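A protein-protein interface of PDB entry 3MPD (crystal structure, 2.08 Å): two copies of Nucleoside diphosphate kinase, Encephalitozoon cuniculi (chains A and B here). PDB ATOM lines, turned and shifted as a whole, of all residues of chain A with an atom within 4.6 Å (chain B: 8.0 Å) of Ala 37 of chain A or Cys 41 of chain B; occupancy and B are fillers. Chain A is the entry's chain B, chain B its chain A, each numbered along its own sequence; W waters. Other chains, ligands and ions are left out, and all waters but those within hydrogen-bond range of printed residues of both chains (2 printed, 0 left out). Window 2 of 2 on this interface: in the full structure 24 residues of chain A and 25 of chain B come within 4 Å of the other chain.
The side-chain hydroxyl (OG) of Ser 39 of chain B is in hydrogen-bond range of the side-chain hydroxyl (OG) of Ser 39 of chain A (2.9 Å).
The side-chain sulfur (SD) of Met 73 of chain B sits close to the backbone carbonyl oxygen (O) of Leu 36 of chain A, at 3.6 Å.
O of Ala 76 of chain B lies within hydrogen-bond range of N of Lys 40 of chain B (2.8 Å).
N of Ala 37 of chain A lies within hydrogen-bond range of O of Val 78 of chain A (2.9 Å).
The backbone carbonyl oxygen of Ala 38 of chain A is in hydrogen-bond range of the backbone NH of Val 78 of chain A.
Among the printed residues, merely in contact across the chains: Ser 39 of chain A with Lys 40 of chain B (3.6 Å), Ala 37 of chain A with Cys 41 of chain B (3.8 Å), Ala 38 of chain A with Cys 41 of chain B (3.8 Å), Leu 36 of chain A with Cys 41 of chain B (3.8 Å), Leu 36 of chain A with Ile 22 of chain B (3.9 Å), Ser 39 of chain A with Leu 75 of chain B (3.9 Å) and Ser 39 of chain A with Cys 41 of chain B (3.9 Å).
Ala 37 of chain A touches just one residue of chain B: Cys 41 (3.8 Å).
Of chain A, only Leu 36 (3.8 Å), Ala 37 (3.8 Å), Ala 38 (3.8 Å) and Ser 39 (3.9 Å) come within 4 Å of Cys 41 of chain B.
Printed residues of chain A within 4 Å of Ile 22 of chain B: Leu 36 (3.9 Å).
Of the printed residues of chain B, Leu 36 of chain A touches Ile 22 (3.9 Å), Cys 41 (3.8 Å) and Met 73 (3.3 Å).
Trp 134 of chain B touches none of the printed residues of chain A.
Val 78 of chain A touches none of the printed residues of chain B.
The nearest printed residue of chain B that does not touch Ala 37 of chain A is Met 73 of chain B (4.5 Å).
The nearest printed residue of chain B that does not touch Ser 39 of chain A is Ala 76 of chain B (6.5 Å).
Printed residues of chain B that touch a printed residue of chain A: Ile 22, Ser 39, Lys 40, Cys 41, Met 73 and Leu 75.
Hydrophobic or aromatic side chains of chain B that line the printed part of chain A: Ile 22, Met 73 and Leu 75.
Printed residues of chain A that touch a printed residue of chain B: Leu 36, Ala 37, Ala 38 and Ser 39.
Hydrophobic or aromatic side chains of chain A within 4 Å of the printed part of chain B: Leu 36.
Among the printed residues, 9 pairs touch across the chains.
Among the printed residues, no Asp or Glu carboxylate lies within 4 Å of a Lys or Arg side-chain nitrogen of the other chain.
Ser 39 of chain B touches its own counterpart, Ser 39 of chain A.
Water W2 bridges the backbone carbonyl oxygen of Ser 39 of chain B and the backbone carbonyl oxygen of Ser 39 of chain A.
Water W1 lies within hydrogen-bond range of the backbone carbonyl oxygen of Ser 39 of chain A (3.0 Å) and the backbone NH of Cys 41 of chain B (3.0 Å).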
ATOM      1  N   TYR A  35      -5.938  10.217 -10.067  1.00  0.00           N
ATOM      2  CA  TYR A  35      -5.430   9.020 -10.691  1.00  0.00           C
ATOM      3  C   TYR A  35      -4.154   8.534 -10.022  1.00  0.00           C
ATOM      4  O   TYR A  35      -3.172   9.258  -9.963  1.00  0.00           O
ATOM      5  CB  TYR A  35      -5.124   9.309 -12.180  1.00  0.00           C
ATOM      6  CG  TYR A  35      -6.368   9.693 -12.943  1.00  0.00           C
ATOM      7  CD1 TYR A  35      -7.284   8.712 -13.352  1.00  0.00           C
ATOM      8  CD2 TYR A  35      -6.656  11.034 -13.238  1.00  0.00           C
ATOM      9  CE1 TYR A  35      -8.450   9.048 -14.050  1.00  0.00           C
ATOM     10  CE2 TYR A  35      -7.829  11.385 -13.934  1.00  0.00           C
ATOM     11  CZ  TYR A  35      -8.725  10.384 -14.324  1.00  0.00           C
ATOM     12  OH  TYR A  35      -9.887  10.702 -15.017  1.00  0.00           O
ATOM     13  N   LEU A  36      -4.144   7.288  -9.560  1.00  0.00           N
ATOM     14  CA  LEU A  36      -2.897   6.673  -9.109  1.00  0.00           C
ATOM     15  C   LEU A  36      -1.967   6.428 -10.291  1.00  0.00           C
ATOM     16  O   LEU A  36      -2.385   5.835 -11.301  1.00  0.00           O
ATOM     17  CB  LEU A  36      -3.207   5.364  -8.371  1.00  0.00           C
ATOM     18  CG  LEU A  36      -2.014   4.631  -7.784  1.00  0.00           C
ATOM     19  CD1 LEU A  36      -1.376   5.392  -6.638  1.00  0.00           C
ATOM     20  CD2 LEU A  36      -2.467   3.254  -7.384  1.00  0.00           C
ATOM     21  N   ALA A  37      -0.721   6.917 -10.166  1.00  0.00           N
ATOM     22  CA  ALA A  37       0.327   6.833 -11.205  1.00  0.00           C
ATOM     23  C   ALA A  37       1.553   6.032 -10.784  1.00  0.00           C
ATOM     24  O   ALA A  37       2.248   5.501 -11.620  1.00  0.00           O
ATOM     25  CB  ALA A  37       0.776   8.238 -11.669  1.00  0.00           C
ATOM     26  N   ALA A  38       1.829   5.980  -9.490  1.00  0.00           N
ATOM     27  CA  ALA A  38       2.961   5.237  -8.987  1.00  0.00           C
ATOM     28  C   ALA A  38       2.672   4.824  -7.563  1.00  0.00           C
ATOM     29  O   ALA A  38       1.899   5.480  -6.864  1.00  0.00           O
ATOM     30  CB  ALA A  38       4.246   6.082  -9.079  1.00  0.00           C
ATOM     31  N   SER A  39       3.272   3.705  -7.164  1.00  0.00           N
ATOM     32  CA  SER A  39       3.077   3.060  -5.857  1.00  0.00           C
ATOM     33  C   SER A  39       4.366   2.309  -5.588  1.00  0.00           C
ATOM     34  O   SER A  39       4.922   1.654  -6.496  1.00  0.00           O
ATOM     35  CB  SER A  39       1.904   2.066  -5.890  1.00  0.00           C
ATOM     36  OG  SER A  39       1.455   1.750  -4.562  1.00  0.00           O
ATOM     37  N   VAL A  78       2.177   8.377  -6.214  1.00  0.00           N
ATOM     38  CA  VAL A  78       1.962   9.606  -6.950  1.00  0.00           C
ATOM     39  C   VAL A  78       0.517   9.610  -7.380  1.00  0.00           C
ATOM     40  O   VAL A  78       0.061   8.640  -7.960  1.00  0.00           O
ATOM     41  CB  VAL A  78       2.862   9.676  -8.212  1.00  0.00           C
ATOM     42  CG1 VAL A  78       2.534  10.925  -9.057  1.00  0.00           C
ATOM     43  CG2 VAL A  78       4.344   9.650  -7.821  1.00  0.00           C
ATOM     44  N   VAL A  80      -2.370  12.015  -9.641  1.00  0.00           N
ATOM     45  CA  VAL A  80      -2.323  12.964 -10.753  1.00  0.00           C
ATOM     46  C   VAL A  80      -3.731  13.489 -11.025  1.00  0.00           C
ATOM     47  O   VAL A  80      -4.730  12.755 -10.897  1.00  0.00           O
ATOM     48  CB  VAL A  80      -1.744  12.274 -12.066  1.00  0.00           C
ATOM     49  CG1 VAL A  80      -1.707  13.240 -13.293  1.00  0.00           C
ATOM     50  CG2 VAL A  80      -0.356  11.716 -11.818  1.00  0.00           C
ATOM     51  N   VAL A 139       8.305   8.119 -13.902  1.00  0.00           N
ATOM     52  CA  VAL A 139       6.921   7.702 -13.725  1.00  0.00           C
ATOM     53  C   VAL A 139       6.216   7.846 -15.071  1.00  0.00           C
ATOM     54  O   VAL A 139       6.232   8.918 -15.691  1.00  0.00           O
ATOM     55  CB  VAL A 139       6.212   8.548 -12.667  1.00  0.00           C
ATOM     56  CG1 VAL A 139       4.717   8.166 -12.571  1.00  0.00           C
ATOM     57  CG2 VAL A 139       6.913   8.392 -11.328  1.00  0.00           C
ATOM     58  N   VAL A 142      -0.105   8.538 -17.169  1.00  0.00           N
ATOM     59  CA  VAL A 142      -1.241   7.742 -16.767  1.00  0.00           C
ATOM     60  C   VAL A 142      -2.404   8.001 -17.719  1.00  0.00           C
ATOM     61  O   VAL A 142      -2.522   9.093 -18.285  1.00  0.00           O
ATOM     62  CB  VAL A 142      -1.588   7.991 -15.273  1.00  0.00           C
ATOM     63  CG1 VAL A 142      -2.283   9.334 -15.068  1.00  0.00           C
ATOM     64  CG2 VAL A 142      -2.419   6.866 -14.736  1.00  0.00           C
ATOM     65  N   ILE B  17      -8.937  -1.125 -12.252  1.00  0.00           N
ATOM     66  CA  ILE B  17      -8.354   0.192 -11.954  1.00  0.00           C
ATOM     67  C   ILE B  17      -9.308   1.292 -12.438  1.00  0.00           C
ATOM     68  O   ILE B  17      -9.619   2.251 -11.713  1.00  0.00           O
ATOM     69  CB  ILE B  17      -6.967   0.391 -12.679  1.00  0.00           C
ATOM     70  CG1 ILE B  17      -5.930  -0.664 -12.246  1.00  0.00           C
ATOM     71  CG2 ILE B  17      -6.443   1.792 -12.438  1.00  0.00           C
ATOM     72  CD1 ILE B  17      -5.623  -0.656 -10.772  1.00  0.00           C
ATOM     73  N   ILE B  22      -9.723  -0.002  -6.511  1.00  0.00           N
ATOM     74  CA  ILE B  22      -8.490  -0.198  -5.738  1.00  0.00           C
ATOM     75  C   ILE B  22      -8.731  -0.292  -4.216  1.00  0.00           C
ATOM     76  O   ILE B  22      -8.309  -1.263  -3.594  1.00  0.00           O
ATOM     77  CB  ILE B  22      -7.392   0.868  -6.039  1.00  0.00           C
ATOM     78  CG1 ILE B  22      -7.001   0.836  -7.527  1.00  0.00           C
ATOM     79  CG2 ILE B  22      -6.101   0.611  -5.153  1.00  0.00           C
ATOM     80  CD1 ILE B  22      -6.104   2.058  -7.930  1.00  0.00           C
ATOM     81  N   SER B  39       4.430  -3.203  -3.979  1.00  0.00           N
ATOM     82  CA  SER B  39       3.397  -2.498  -4.721  1.00  0.00           C
ATOM     83  C   SER B  39       4.079  -1.829  -5.900  1.00  0.00           C
ATOM     84  O   SER B  39       5.183  -1.242  -5.739  1.00  0.00           O
ATOM     85  CB  SER B  39       2.805  -1.404  -3.843  1.00  0.00           C
ATOM     86  OG  SER B  39       1.492  -1.089  -4.253  1.00  0.00           O
ATOM     87  N   LYS B  40       3.463  -1.916  -7.076  1.00  0.00           N
ATOM     88  CA  LYS B  40       4.026  -1.305  -8.267  1.00  0.00           C
ATOM     89  C   LYS B  40       2.919  -1.112  -9.297  1.00  0.00           C
ATOM     90  O   LYS B  40       2.161  -2.037  -9.568  1.00  0.00           O
ATOM     91  CB  LYS B  40       5.158  -2.194  -8.862  1.00  0.00           C
ATOM     92  CG  LYS B  40       5.872  -1.594 -10.055  1.00  0.00           C
ATOM     93  CD  LYS B  40       6.953  -2.521 -10.637  1.00  0.00           C
ATOM     94  CE  LYS B  40       7.620  -1.829 -11.828  1.00  0.00           C
ATOM     95  NZ  LYS B  40       8.060  -2.754 -12.937  1.00  0.00           N
ATOM     96  N   CYS B  41       2.846   0.094  -9.858  1.00  0.00           N
ATOM     97  CA  CYS B  41       1.991   0.384 -11.004  1.00  0.00           C
ATOM     98  C   CYS B  41       2.775   0.073 -12.274  1.00  0.00           C
ATOM     99  O   CYS B  41       3.883   0.589 -12.460  1.00  0.00           O
ATOM    100  CB  CYS B  41       1.582   1.858 -11.019  1.00  0.00           C
ATOM    101  SG  CYS B  41       0.523   2.377  -9.619  1.00  0.00           S
ATOM    102  N   VAL B  42       2.207  -0.769 -13.145  1.00  0.00           N
ATOM    103  CA  VAL B  42       2.885  -1.124 -14.410  1.00  0.00           C
ATOM    104  C   VAL B  42       1.906  -1.197 -15.565  1.00  0.00           C
ATOM    105  O   VAL B  42       0.789  -1.681 -15.389  1.00  0.00           O
ATOM    106  CB  VAL B  42       3.530  -2.539 -14.378  1.00  0.00           C
ATOM    107  CG1 VAL B  42       4.730  -2.603 -15.370  1.00  0.00           C
ATOM    108  CG2 VAL B  42       3.957  -2.926 -12.991  1.00  0.00           C
ATOM    109  N   ILE B  43       2.364  -0.745 -16.739  1.00  0.00           N
ATOM    110  CA  ILE B  43       1.712  -0.987 -18.009  1.00  0.00           C
ATOM    111  C   ILE B  43       2.345  -2.301 -18.485  1.00  0.00           C
ATOM    112  O   ILE B  43       3.505  -2.296 -18.859  1.00  0.00           O
ATOM    113  CB  ILE B  43       2.053   0.139 -19.020  1.00  0.00           C
ATOM    114  CG1 ILE B  43       1.875   1.528 -18.373  1.00  0.00           C
ATOM    115  CG2 ILE B  43       1.281  -0.043 -20.367  1.00  0.00           C
ATOM    116  CD1 ILE B  43       3.161   2.028 -17.603  1.00  0.00           C
ATOM    117  N   PRO B  44       1.603  -3.426 -18.435  1.00  0.00           N
ATOM    118  CA  PRO B  44       2.233  -4.710 -18.727  1.00  0.00           C
ATOM    119  C   PRO B  44       2.773  -4.828 -20.173  1.00  0.00           C
ATOM    120  O   PRO B  44       2.135  -4.367 -21.118  1.00  0.00           O
ATOM    121  CB  PRO B  44       1.107  -5.719 -18.514  1.00  0.00           C
ATOM    122  CG  PRO B  44       0.113  -5.032 -17.611  1.00  0.00           C
ATOM    123  CD  PRO B  44       0.197  -3.583 -18.014  1.00  0.00           C
ATOM    124  N   MET B  73      -2.856   0.249 -17.140  1.00  0.00           N
ATOM    125  CA  MET B  73      -2.055   0.083 -15.936  1.00  0.00           C
ATOM    126  C   MET B  73      -2.678  -0.969 -15.023  1.00  0.00           C
ATOM    127  O   MET B  73      -3.924  -1.035 -14.888  1.00  0.00           O
ATOM    128  CB  MET B  73      -1.992   1.424 -15.216  1.00  0.00           C
ATOM    129  CG  MET B  73      -0.884   1.589 -14.191  1.00  0.00           C
ATOM    130  SD  MET B  73      -1.198   3.129 -13.315  1.00  0.00           S
ATOM    131  CE  MET B  73      -2.313   2.573 -12.027  1.00  0.00           C
ATOM    132  N   VAL B  74      -1.816  -1.792 -14.416  1.00  0.00           N
ATOM    133  CA  VAL B  74      -2.223  -2.750 -13.392  1.00  0.00           C
ATOM    134  C   VAL B  74      -1.560  -2.307 -12.098  1.00  0.00           C
ATOM    135  O   VAL B  74      -0.553  -1.600 -12.144  1.00  0.00           O
ATOM    136  CB  VAL B  74      -1.799  -4.238 -13.716  1.00  0.00           C
ATOM    137  CG1 VAL B  74      -2.519  -4.765 -14.962  1.00  0.00           C
ATOM    138  CG2 VAL B  74      -0.295  -4.390 -13.884  1.00  0.00           C
ATOM    139  N   LEU B  75      -2.129  -2.704 -10.955  1.00  0.00           N
ATOM    140  CA  LEU B  75      -1.450  -2.572  -9.656  1.00  0.00           C
ATOM    141  C   LEU B  75      -0.972  -3.933  -9.149  1.00  0.00           C
ATOM    142  O   LEU B  75      -1.783  -4.780  -8.728  1.00  0.00           O
ATOM    143  CB  LEU B  75      -2.334  -1.861  -8.610  1.00  0.00           C
ATOM    144  CG  LEU B  75      -1.723  -1.591  -7.217  1.00  0.00           C
ATOM    145  CD1 LEU B  75      -0.503  -0.659  -7.321  1.00  0.00           C
ATOM    146  CD2 LEU B  75      -2.767  -0.995  -6.263  1.00  0.00           C
ATOM    147  N   ALA B  76       0.337  -4.136  -9.211  1.00  0.00           N
ATOM    148  CA  ALA B  76       0.963  -5.388  -8.814  1.00  0.00           C
ATOM    149  C   ALA B  76       1.419  -5.315  -7.355  1.00  0.00           C
ATOM    150  O   ALA B  76       2.092  -4.351  -6.964  1.00  0.00           O
ATOM    151  CB  ALA B  76       2.150  -5.688  -9.718  1.00  0.00           C
ATOM    152  N   MET B  77       1.081  -6.341  -6.572  1.00  0.00           N
ATOM    153  CA  MET B  77       1.374  -6.354  -5.130  1.00  0.00           C
ATOM    154  C   MET B  77       1.875  -7.693  -4.652  1.00  0.00           C
ATOM    155  O   MET B  77       1.546  -8.735  -5.228  1.00  0.00           O
ATOM    156  CB  MET B  77       0.076  -6.055  -4.310  1.00  0.00           C
ATOM    157  CG  MET B  77      -0.431  -4.641  -4.469  1.00  0.00           C
ATOM    158  SD  MET B  77      -2.135  -4.344  -3.905  1.00  0.00           S
ATOM    159  CE  MET B  77      -3.093  -5.089  -5.201  1.00  0.00           C
ATOM    160  N   TRP B 134       7.343  -9.949 -12.050  1.00  0.00           N
ATOM    161  CA  TRP B 134       6.746  -8.612 -12.018  1.00  0.00           C
ATOM    162  C   TRP B 134       7.413  -7.592 -11.094  1.00  0.00           C
ATOM    163  O   TRP B 134       7.370  -6.390 -11.371  1.00  0.00           O
ATOM    164  CB  TRP B 134       5.275  -8.711 -11.585  1.00  0.00           C
ATOM    165  CG  TRP B 134       4.389  -9.392 -12.551  1.00  0.00           C
ATOM    166  CD1 TRP B 134       4.060 -10.720 -12.573  1.00  0.00           C
ATOM    167  CD2 TRP B 134       3.692  -8.788 -13.630  1.00  0.00           C
ATOM    168  NE1 TRP B 134       3.192 -10.976 -13.602  1.00  0.00           N
ATOM    169  CE2 TRP B 134       2.949  -9.806 -14.270  1.00  0.00           C
ATOM    170  CE3 TRP B 134       3.614  -7.479 -14.121  1.00  0.00           C
ATOM    171  CZ2 TRP B 134       2.129  -9.556 -15.364  1.00  0.00           C
ATOM    172  CZ3 TRP B 134       2.813  -7.227 -15.213  1.00  0.00           C
ATOM    173  CH2 TRP B 134       2.078  -8.266 -15.828  1.00  0.00           C
ATOM    174  N   ILE B 135       7.973  -8.066  -9.980  1.00  0.00           N
ATOM    175  CA  ILE B 135       8.458  -7.182  -8.909  1.00  0.00           C
ATOM    176  C   ILE B 135       9.978  -7.190  -8.813  1.00  0.00           C
ATOM    177  O   ILE B 135      10.600  -6.128  -8.822  1.00  0.00           O
ATOM    178  CB  ILE B 135       7.875  -7.571  -7.517  1.00  0.00           C
ATOM    179  CG1 ILE B 135       6.359  -7.641  -7.551  1.00  0.00           C
ATOM    180  CG2 ILE B 135       8.338  -6.590  -6.445  1.00  0.00           C
ATOM    181  CD1 ILE B 135       5.684  -6.298  -7.731  1.00  0.00           C
HETATM  182  O   HOH W   1       4.795   2.357  -9.414  1.00  0.00           O
HETATM  183  O   HOH W   2       7.132   0.041  -7.120  1.00  0.00           O
